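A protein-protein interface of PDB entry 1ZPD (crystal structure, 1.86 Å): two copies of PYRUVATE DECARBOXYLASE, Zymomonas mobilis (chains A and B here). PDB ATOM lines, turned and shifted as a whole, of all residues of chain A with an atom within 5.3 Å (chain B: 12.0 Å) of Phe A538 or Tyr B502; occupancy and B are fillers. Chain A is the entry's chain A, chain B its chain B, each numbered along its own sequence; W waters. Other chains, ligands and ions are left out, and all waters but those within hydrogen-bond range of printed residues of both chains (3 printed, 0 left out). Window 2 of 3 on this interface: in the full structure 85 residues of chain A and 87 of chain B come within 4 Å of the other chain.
The backbone carbonyl oxygen (O) of Asn A466 sits at hydrogen-bond distance from the side-chain hydroxyl (OH) of Tyr B502. The side-chain carboxylate of Asp B503 lies within hydrogen-bond range of the side-chain hydroxyl of Tyr A468 (2.7 Å). The side-chain amide nitrogen (ND2) of Asn A486 lies close to the backbone NH (N) of Tyr B502, 3.4 Å away. The side-chain carboxylate of Asp B503 lies within hydrogen-bond range of the backbone NH of Asn A486, 3.0 Å away. OH of Tyr B502 lies within hydrogen-bond range of O of Ile A539 (3.1 Å). O of Asn A486 lies close to O of Phe B496, 3.5 Å away.
N of Tyr A468 is in hydrogen-bond range of OD1 of Asn A466. The side-chain amide oxygen of Asn A486 is in hydrogen-bond range of the side-chain amide nitrogen of Asn A466, 3.0 Å away. The side-chain amide nitrogen of Asn A466 sits at hydrogen-bond distance from the side-chain carboxylate of Glu A536 (2.9 Å). The backbone carbonyl oxygen of Cys A537 lies within hydrogen-bond range of the backbone NH of Asn A466 (2.7 Å). The backbone NH (N) of Ile A539 lies within hydrogen-bond range of the backbone carbonyl oxygen (O) of Asn A466 (3.3 Å). N of Phe A538 sits at hydrogen-bond distance from O of Ala A512, at 3.1 Å.
CG of Tyr B502 touches CG of Tyr A468, 3.6 Å away. ND2 of Asn A486 touches CA of Gly B501 (3.9 Å). Tyr B502 touches Phe A538.
Of chain B, only Tyr B502 (3.8 Å) comes within 4 Å of Phe A538. Tyr B502 touches just these residues of chain A: Asn A466 (2.8 Å), Tyr A468 (3.6 Å), Asn A486 (3.4 Å), Phe A538 (3.8 Å) and Ile A539 (3.1 Å). Tyr A468 touches two residues of chain B. Of chain B, only Phe B496 (3.5 Å), Gly B501 (3.9 Å), Tyr B502 (3.4 Å) and Asp B503 (3.0 Å) come within 4 Å of Asn A486. No residue of chain B comes within 4 Å of Lys A513. No residue of chain B comes within 4 Å of Cys A537. Of the printed residues of chain B, Ile A539 touches Tyr B502. No residue of chain B comes within 4 Å of Gly A540. Printed residues of chain A within 4 Å of Gly B501: Asn A486 (3.9 Å). Of the printed residues of chain A, Asp B503 touches Tyr A468 and Asn A486.
Hydrophobic or aromatic side chains of chain A that line the printed part of chain B: Tyr A468 and Phe A538. Of the 15 printed residues of chain B, 4 touch a printed residue of chain A. Among the printed residues, 9 pairs touch across the chains.
No position is printed for both chains. Of the 9 pairs that touch across the chains among the printed residues, none has its exchanged pair printed and touching as well.
Water W2 lies within hydrogen-bond range of O of Gly B498 (2.5 Å), OD1 of Asp B503 (2.7 Å), ND2 of Asn A486 (2.9 Å) and N of Tyr B502 (3.5 Å). Water W1 lies within hydrogen-bond range of NZ of Lys A513 (2.8 Å) and O of Gly B500 (3.1 Å). Water W3 bridges OH of Tyr B502 and O of Ile A539.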
ATOM      1  N   LEU A 365     -30.477 -17.533  20.306  1.00  0.00           N
ATOM      2  CA  LEU A 365     -31.463 -17.611  21.390  1.00  0.00           C
ATOM      3  C   LEU A 365     -31.526 -16.318  22.190  1.00  0.00           C
ATOM      4  O   LEU A 365     -30.481 -15.708  22.482  1.00  0.00           O
ATOM      5  CB  LEU A 365     -31.130 -18.770  22.323  1.00  0.00           C
ATOM      6  CG  LEU A 365     -32.147 -19.153  23.409  1.00  0.00           C
ATOM      7  CD1 LEU A 365     -33.509 -19.507  22.793  1.00  0.00           C
ATOM      8  CD2 LEU A 365     -31.612 -20.334  24.214  1.00  0.00           C
ATOM      9  N   ASN A 466     -27.638 -19.858  31.112  1.00  0.00           N
ATOM     10  CA  ASN A 466     -26.210 -19.483  31.112  1.00  0.00           C
ATOM     11  C   ASN A 466     -26.000 -18.118  30.477  1.00  0.00           C
ATOM     12  O   ASN A 466     -25.708 -17.943  29.290  1.00  0.00           O
ATOM     13  CB  ASN A 466     -25.347 -20.565  30.448  1.00  0.00           C
ATOM     14  CG  ASN A 466     -23.849 -20.355  30.703  1.00  0.00           C
ATOM     15  OD1 ASN A 466     -23.469 -19.378  31.361  1.00  0.00           O
ATOM     16  ND2 ASN A 466     -22.988 -21.220  30.190  1.00  0.00           N
ATOM     17  N   ASN A 467     -26.141 -17.080  31.310  1.00  0.00           N
ATOM     18  CA  ASN A 467     -25.833 -15.715  30.921  1.00  0.00           C
ATOM     19  C   ASN A 467     -24.471 -15.273  31.495  1.00  0.00           C
ATOM     20  O   ASN A 467     -24.197 -14.081  31.575  1.00  0.00           O
ATOM     21  CB  ASN A 467     -26.962 -14.768  31.343  1.00  0.00           C
ATOM     22  CG  ASN A 467     -27.310 -14.807  32.822  1.00  0.00           C
ATOM     23  OD1 ASN A 467     -26.571 -15.388  33.633  1.00  0.00           O
ATOM     24  ND2 ASN A 467     -28.418 -14.186  33.213  1.00  0.00           N
ATOM     25  N   TYR A 468     -23.639 -16.216  31.908  1.00  0.00           N
ATOM     26  CA  TYR A 468     -22.266 -15.923  32.367  1.00  0.00           C
ATOM     27  C   TYR A 468     -22.222 -14.910  33.508  1.00  0.00           C
ATOM     28  O   TYR A 468     -21.594 -13.855  33.365  1.00  0.00           O
ATOM     29  CB  TYR A 468     -21.377 -15.518  31.186  1.00  0.00           C
ATOM     30  CG  TYR A 468     -19.866 -15.607  31.418  1.00  0.00           C
ATOM     31  CD1 TYR A 468     -19.285 -16.602  32.195  1.00  0.00           C
ATOM     32  CD2 TYR A 468     -19.019 -14.663  30.843  1.00  0.00           C
ATOM     33  CE1 TYR A 468     -17.904 -16.662  32.391  1.00  0.00           C
ATOM     34  CE2 TYR A 468     -17.636 -14.709  31.032  1.00  0.00           C
ATOM     35  CZ  TYR A 468     -17.089 -15.712  31.806  1.00  0.00           C
ATOM     36  OH  TYR A 468     -15.715 -15.768  31.999  1.00  0.00           O
ATOM     37  N   ASN A 486     -17.041 -19.877  34.246  1.00  0.00           N
ATOM     38  CA  ASN A 486     -18.033 -20.652  33.477  1.00  0.00           C
ATOM     39  C   ASN A 486     -17.739 -22.142  33.560  1.00  0.00           C
ATOM     40  O   ASN A 486     -16.590 -22.540  33.771  1.00  0.00           O
ATOM     41  CB  ASN A 486     -18.030 -20.213  31.998  1.00  0.00           C
ATOM     42  CG  ASN A 486     -19.137 -20.878  31.171  1.00  0.00           C
ATOM     43  OD1 ASN A 486     -20.313 -20.811  31.538  1.00  0.00           O
ATOM     44  ND2 ASN A 486     -18.750 -21.520  30.067  1.00  0.00           N
ATOM     45  N   LYS A 511     -27.131 -28.550  24.907  1.00  0.00           N
ATOM     46  CA  LYS A 511     -26.890 -27.125  24.767  1.00  0.00           C
ATOM     47  C   LYS A 511     -27.894 -26.514  23.786  1.00  0.00           C
ATOM     48  O   LYS A 511     -28.281 -27.167  22.801  1.00  0.00           O
ATOM     49  CB  LYS A 511     -25.442 -26.858  24.304  1.00  0.00           C
ATOM     50  CG  LYS A 511     -24.381 -27.329  25.317  1.00  0.00           C
ATOM     51  CD  LYS A 511     -22.968 -26.981  24.844  1.00  0.00           C
ATOM     52  CE  LYS A 511     -21.883 -27.594  25.731  1.00  0.00           C
ATOM     53  NZ  LYS A 511     -21.719 -26.843  27.024  1.00  0.00           N
ATOM     54  N   ALA A 512     -28.344 -25.302  24.062  1.00  0.00           N
ATOM     55  CA  ALA A 512     -29.248 -24.577  23.181  1.00  0.00           C
ATOM     56  C   ALA A 512     -28.767 -23.146  22.969  1.00  0.00           C
ATOM     57  O   ALA A 512     -28.771 -22.321  23.882  1.00  0.00           O
ATOM     58  CB  ALA A 512     -30.685 -24.558  23.736  1.00  0.00           C
ATOM     59  N   LYS A 513     -28.428 -22.839  21.708  1.00  0.00           N
ATOM     60  CA  LYS A 513     -27.947 -21.529  21.323  1.00  0.00           C
ATOM     61  C   LYS A 513     -28.882 -20.827  20.337  1.00  0.00           C
ATOM     62  O   LYS A 513     -28.683 -19.686  19.925  1.00  0.00           O
ATOM     63  CB  LYS A 513     -26.522 -21.620  20.730  1.00  0.00           C
ATOM     64  CG  LYS A 513     -25.502 -22.207  21.710  1.00  0.00           C
ATOM     65  CD  LYS A 513     -24.065 -22.095  21.211  1.00  0.00           C
ATOM     66  CE  LYS A 513     -23.087 -22.481  22.329  1.00  0.00           C
ATOM     67  NZ  LYS A 513     -21.870 -23.184  21.818  1.00  0.00           N
ATOM     68  N   GLU A 536     -28.781 -26.478  28.704  1.00  0.00           N
ATOM     69  CA  GLU A 536     -27.951 -25.290  28.931  1.00  0.00           C
ATOM     70  C   GLU A 536     -28.267 -24.235  27.877  1.00  0.00           C
ATOM     71  O   GLU A 536     -27.918 -24.366  26.694  1.00  0.00           O
ATOM     72  CB  GLU A 536     -26.462 -25.698  28.944  1.00  0.00           C
ATOM     73  CG  GLU A 536     -25.526 -24.518  29.216  1.00  0.00           C
ATOM     74  CD  GLU A 536     -24.049 -24.864  29.053  1.00  0.00           C
ATOM     75  OE1 GLU A 536     -23.698 -26.019  28.734  1.00  0.00           O
ATOM     76  OE2 GLU A 536     -23.223 -23.951  29.254  1.00  0.00           O
ATOM     77  N   CYS A 537     -28.978 -23.189  28.304  1.00  0.00           N
ATOM     78  CA  CYS A 537     -29.436 -22.123  27.422  1.00  0.00           C
ATOM     79  C   CYS A 537     -28.465 -20.948  27.422  1.00  0.00           C
ATOM     80  O   CYS A 537     -28.202 -20.363  28.495  1.00  0.00           O
ATOM     81  CB  CYS A 537     -30.856 -21.676  27.837  1.00  0.00           C
ATOM     82  SG  CYS A 537     -32.055 -23.058  27.849  1.00  0.00           S
ATOM     83  N   PHE A 538     -27.956 -20.575  26.250  1.00  0.00           N
ATOM     84  CA  PHE A 538     -26.957 -19.514  26.147  1.00  0.00           C
ATOM     85  C   PHE A 538     -27.587 -18.196  25.728  1.00  0.00           C
ATOM     86  O   PHE A 538     -28.118 -18.076  24.605  1.00  0.00           O
ATOM     87  CB  PHE A 538     -25.855 -19.854  25.130  1.00  0.00           C
ATOM     88  CG  PHE A 538     -24.956 -20.992  25.501  1.00  0.00           C
ATOM     89  CD1 PHE A 538     -25.385 -22.305  25.395  1.00  0.00           C
ATOM     90  CD2 PHE A 538     -23.656 -20.753  25.970  1.00  0.00           C
ATOM     91  CE1 PHE A 538     -24.548 -23.353  25.747  1.00  0.00           C
ATOM     92  CE2 PHE A 538     -22.815 -21.794  26.322  1.00  0.00           C
ATOM     93  CZ  PHE A 538     -23.257 -23.096  26.206  1.00  0.00           C
ATOM     94  N   ILE A 539     -27.540 -17.198  26.616  1.00  0.00           N
ATOM     95  CA  ILE A 539     -28.052 -15.866  26.318  1.00  0.00           C
ATOM     96  C   ILE A 539     -27.078 -14.819  26.888  1.00  0.00           C
ATOM     97  O   ILE A 539     -26.197 -15.169  27.688  1.00  0.00           O
ATOM     98  CB  ILE A 539     -29.465 -15.546  26.856  1.00  0.00           C
ATOM     99  CG1 ILE A 539     -29.580 -15.824  28.367  1.00  0.00           C
ATOM    100  CG2 ILE A 539     -30.553 -16.315  26.088  1.00  0.00           C
ATOM    101  CD1 ILE A 539     -30.874 -15.320  29.004  1.00  0.00           C
ATOM    102  N   GLY A 540     -27.235 -13.571  26.478  1.00  0.00           N
ATOM    103  CA  GLY A 540     -26.328 -12.514  26.927  1.00  0.00           C
ATOM    104  C   GLY A 540     -26.639 -12.048  28.355  1.00  0.00           C
ATOM    105  O   GLY A 540     -27.795 -12.076  28.803  1.00  0.00           O
ATOM    106  N   VAL B 454      -9.056 -23.706  39.088  1.00  0.00           N
ATOM    107  CA  VAL B 454      -8.951 -23.569  37.629  1.00  0.00           C
ATOM    108  C   VAL B 454      -8.877 -22.100  37.234  1.00  0.00           C
ATOM    109  O   VAL B 454      -7.993 -21.662  36.488  1.00  0.00           O
ATOM    110  CB  VAL B 454     -10.148 -24.225  36.884  1.00  0.00           C
ATOM    111  CG1 VAL B 454      -9.941 -24.114  35.360  1.00  0.00           C
ATOM    112  CG2 VAL B 454     -10.281 -25.671  37.296  1.00  0.00           C
ATOM    113  N   ARG B 455      -9.780 -21.292  37.775  1.00  0.00           N
ATOM    114  CA  ARG B 455      -9.916 -19.883  37.472  1.00  0.00           C
ATOM    115  C   ARG B 455      -8.628 -19.100  37.778  1.00  0.00           C
ATOM    116  O   ARG B 455      -8.207 -18.266  36.971  1.00  0.00           O
ATOM    117  CB  ARG B 455     -11.049 -19.289  38.332  1.00  0.00           C
ATOM    118  CG  ARG B 455     -11.445 -17.866  37.955  1.00  0.00           C
ATOM    119  CD  ARG B 455     -12.417 -17.326  39.007  1.00  0.00           C
ATOM    120  NE  ARG B 455     -13.172 -16.156  38.561  1.00  0.00           N
ATOM    121  CZ  ARG B 455     -14.261 -15.731  39.218  1.00  0.00           C
ATOM    122  NH1 ARG B 455     -14.672 -16.368  40.315  1.00  0.00           N
ATOM    123  NH2 ARG B 455     -14.924 -14.665  38.785  1.00  0.00           N
ATOM    124  N   GLU B 494     -12.785 -31.223  33.047  1.00  0.00           N
ATOM    125  CA  GLU B 494     -13.154 -30.572  31.779  1.00  0.00           C
ATOM    126  C   GLU B 494     -14.441 -29.757  31.925  1.00  0.00           C
ATOM    127  O   GLU B 494     -14.612 -28.732  31.263  1.00  0.00           O
ATOM    128  CB  GLU B 494     -13.301 -31.555  30.615  1.00  0.00           C
ATOM    129  CG  GLU B 494     -12.000 -32.007  29.982  1.00  0.00           C
ATOM    130  CD  GLU B 494     -10.994 -30.944  29.594  1.00  0.00           C
ATOM    131  OE1 GLU B 494     -11.336 -29.781  29.311  1.00  0.00           O
ATOM    132  OE2 GLU B 494      -9.783 -31.303  29.576  1.00  0.00           O
ATOM    133  N   VAL B 495     -15.368 -30.216  32.779  1.00  0.00           N
ATOM    134  CA  VAL B 495     -16.579 -29.429  33.052  1.00  0.00           C
ATOM    135  C   VAL B 495     -16.188 -28.082  33.646  1.00  0.00           C
ATOM    136  O   VAL B 495     -16.714 -27.052  33.220  1.00  0.00           O
ATOM    137  CB  VAL B 495     -17.531 -30.196  34.000  1.00  0.00           C
ATOM    138  CG1 VAL B 495     -18.593 -29.293  34.605  1.00  0.00           C
ATOM    139  CG2 VAL B 495     -18.175 -31.351  33.222  1.00  0.00           C
ATOM    140  N   PHE B 496     -15.265 -28.059  34.626  1.00  0.00           N
ATOM    141  CA  PHE B 496     -14.819 -26.795  35.214  1.00  0.00           C
ATOM    142  C   PHE B 496     -13.920 -26.005  34.272  1.00  0.00           C
ATOM    143  O   PHE B 496     -13.961 -24.769  34.327  1.00  0.00           O
ATOM    144  CB  PHE B 496     -14.133 -27.060  36.565  1.00  0.00           C
ATOM    145  CG  PHE B 496     -14.987 -27.586  37.690  1.00  0.00           C
ATOM    146  CD1 PHE B 496     -16.354 -27.330  37.769  1.00  0.00           C
ATOM    147  CD2 PHE B 496     -14.389 -28.364  38.690  1.00  0.00           C
ATOM    148  CE1 PHE B 496     -17.106 -27.826  38.816  1.00  0.00           C
ATOM    149  CE2 PHE B 496     -15.152 -28.861  39.749  1.00  0.00           C
ATOM    150  CZ  PHE B 496     -16.508 -28.594  39.808  1.00  0.00           C
ATOM    151  N   ASN B 497     -13.180 -26.622  33.339  1.00  0.00           N
ATOM    152  CA  ASN B 497     -12.530 -25.824  32.292  1.00  0.00           C
ATOM    153  C   ASN B 497     -13.521 -25.064  31.412  1.00  0.00           C
ATOM    154  O   ASN B 497     -13.378 -23.865  31.166  1.00  0.00           O
ATOM    155  CB  ASN B 497     -11.681 -26.736  31.380  1.00  0.00           C
ATOM    156  CG  ASN B 497     -10.421 -27.224  32.076  1.00  0.00           C
ATOM    157  OD1 ASN B 497     -10.000 -26.617  33.080  1.00  0.00           O
ATOM    158  ND2 ASN B 497      -9.812 -28.287  31.566  1.00  0.00           N
ATOM    159  N   GLY B 498     -14.526 -25.775  30.867  1.00  0.00           N
ATOM    160  CA  GLY B 498     -15.500 -25.145  29.968  1.00  0.00           C
ATOM    161  C   GLY B 498     -14.857 -24.633  28.676  1.00  0.00           C
ATOM    162  O   GLY B 498     -15.308 -23.607  28.158  1.00  0.00           O
ATOM    163  N   ASN B 499     -13.820 -25.301  28.177  1.00  0.00           N
ATOM    164  CA  ASN B 499     -13.178 -24.836  26.933  1.00  0.00           C
ATOM    165  C   ASN B 499     -14.204 -24.861  25.791  1.00  0.00           C
ATOM    166  O   ASN B 499     -14.961 -25.832  25.664  1.00  0.00           O
ATOM    167  CB  ASN B 499     -11.910 -25.650  26.624  1.00  0.00           C
ATOM    168  CG  ASN B 499     -10.831 -25.387  27.688  1.00  0.00           C
ATOM    169  OD1 ASN B 499     -10.671 -24.252  28.135  1.00  0.00           O
ATOM    170  ND2 ASN B 499     -10.106 -26.417  28.102  1.00  0.00           N
ATOM    171  N   GLY B 500     -14.288 -23.775  25.026  1.00  0.00           N
ATOM    172  CA  GLY B 500     -15.297 -23.647  23.967  1.00  0.00           C
ATOM    173  C   GLY B 500     -16.520 -22.857  24.437  1.00  0.00           C
ATOM    174  O   GLY B 500     -17.421 -22.546  23.636  1.00  0.00           O
ATOM    175  N   GLY B 501     -16.555 -22.525  25.735  1.00  0.00           N
ATOM    176  CA  GLY B 501     -17.670 -21.763  26.303  1.00  0.00           C
ATOM    177  C   GLY B 501     -17.249 -20.300  26.418  1.00  0.00           C
ATOM    178  O   GLY B 501     -16.351 -19.868  25.677  1.00  0.00           O
ATOM    179  N   TYR B 502     -17.766 -19.610  27.427  1.00  0.00           N
ATOM    180  CA  TYR B 502     -17.446 -18.215  27.674  1.00  0.00           C
ATOM    181  C   TYR B 502     -15.993 -17.952  28.113  1.00  0.00           C
ATOM    182  O   TYR B 502     -15.522 -16.827  27.931  1.00  0.00           O
ATOM    183  CB  TYR B 502     -18.380 -17.665  28.757  1.00  0.00           C
ATOM    184  CG  TYR B 502     -19.847 -17.538  28.375  1.00  0.00           C
ATOM    185  CD1 TYR B 502     -20.271 -16.624  27.409  1.00  0.00           C
ATOM    186  CD2 TYR B 502     -20.813 -18.327  28.994  1.00  0.00           C
ATOM    187  CE1 TYR B 502     -21.618 -16.504  27.066  1.00  0.00           C
ATOM    188  CE2 TYR B 502     -22.161 -18.210  28.653  1.00  0.00           C
ATOM    189  CZ  TYR B 502     -22.558 -17.300  27.694  1.00  0.00           C
ATOM    190  OH  TYR B 502     -23.900 -17.180  27.351  1.00  0.00           O
ATOM    191  N   ASP B 503     -15.311 -18.909  28.731  1.00  0.00           N
ATOM    192  CA  ASP B 503     -13.906 -18.702  29.139  1.00  0.00           C
ATOM    193  C   ASP B 503     -13.127 -19.987  28.904  1.00  0.00           C
ATOM    194  O   ASP B 503     -13.456 -20.722  27.951  1.00  0.00           O
ATOM    195  CB  ASP B 503     -13.785 -18.178  30.576  1.00  0.00           C
ATOM    196  CG  ASP B 503     -14.537 -18.956  31.633  1.00  0.00           C
ATOM    197  OD1 ASP B 503     -14.606 -20.199  31.549  1.00  0.00           O
ATOM    198  OD2 ASP B 503     -15.018 -18.330  32.604  1.00  0.00           O
ATOM    199  N   SER B 504     -12.134 -20.304  29.733  1.00  0.00           N
ATOM    200  CA  SER B 504     -11.315 -21.492  29.509  1.00  0.00           C
ATOM    201  C   SER B 504     -10.639 -21.924  30.819  1.00  0.00           C
ATOM    202  O   SER B 504     -10.728 -21.217  31.830  1.00  0.00           O
ATOM    203  CB  SER B 504     -10.235 -21.179  28.452  1.00  0.00           C
ATOM    204  OG  SER B 504      -9.301 -20.244  28.997  1.00  0.00           O
ATOM    205  N   GLY B 505      -9.989 -23.084  30.783  1.00  0.00           N
ATOM    206  CA  GLY B 505      -9.208 -23.550  31.928  1.00  0.00           C
ATOM    207  C   GLY B 505      -8.135 -24.548  31.506  1.00  0.00           C
ATOM    208  O   GLY B 505      -8.252 -25.197  30.455  1.00  0.00           O
ATOM    209  N   ALA B 506      -7.197 -24.833  32.423  1.00  0.00           N
ATOM    210  CA  ALA B 506      -6.098 -25.747  32.135  1.00  0.00           C
ATOM    211  C   ALA B 506      -6.050 -26.900  33.122  1.00  0.00           C
ATOM    212  O   ALA B 506      -4.995 -27.519  33.337  1.00  0.00           O
ATOM    213  CB  ALA B 506      -4.766 -24.978  32.123  1.00  0.00           C
HETATM  214  O   HOH W   1     -20.271 -23.592  24.050  1.00  0.00           O
HETATM  215  O   HOH W   2     -15.907 -21.586  29.577  1.00  0.00           O
HETATM  216  O   HOH W   3     -24.289 -15.569  25.033  1.00  0.00           O
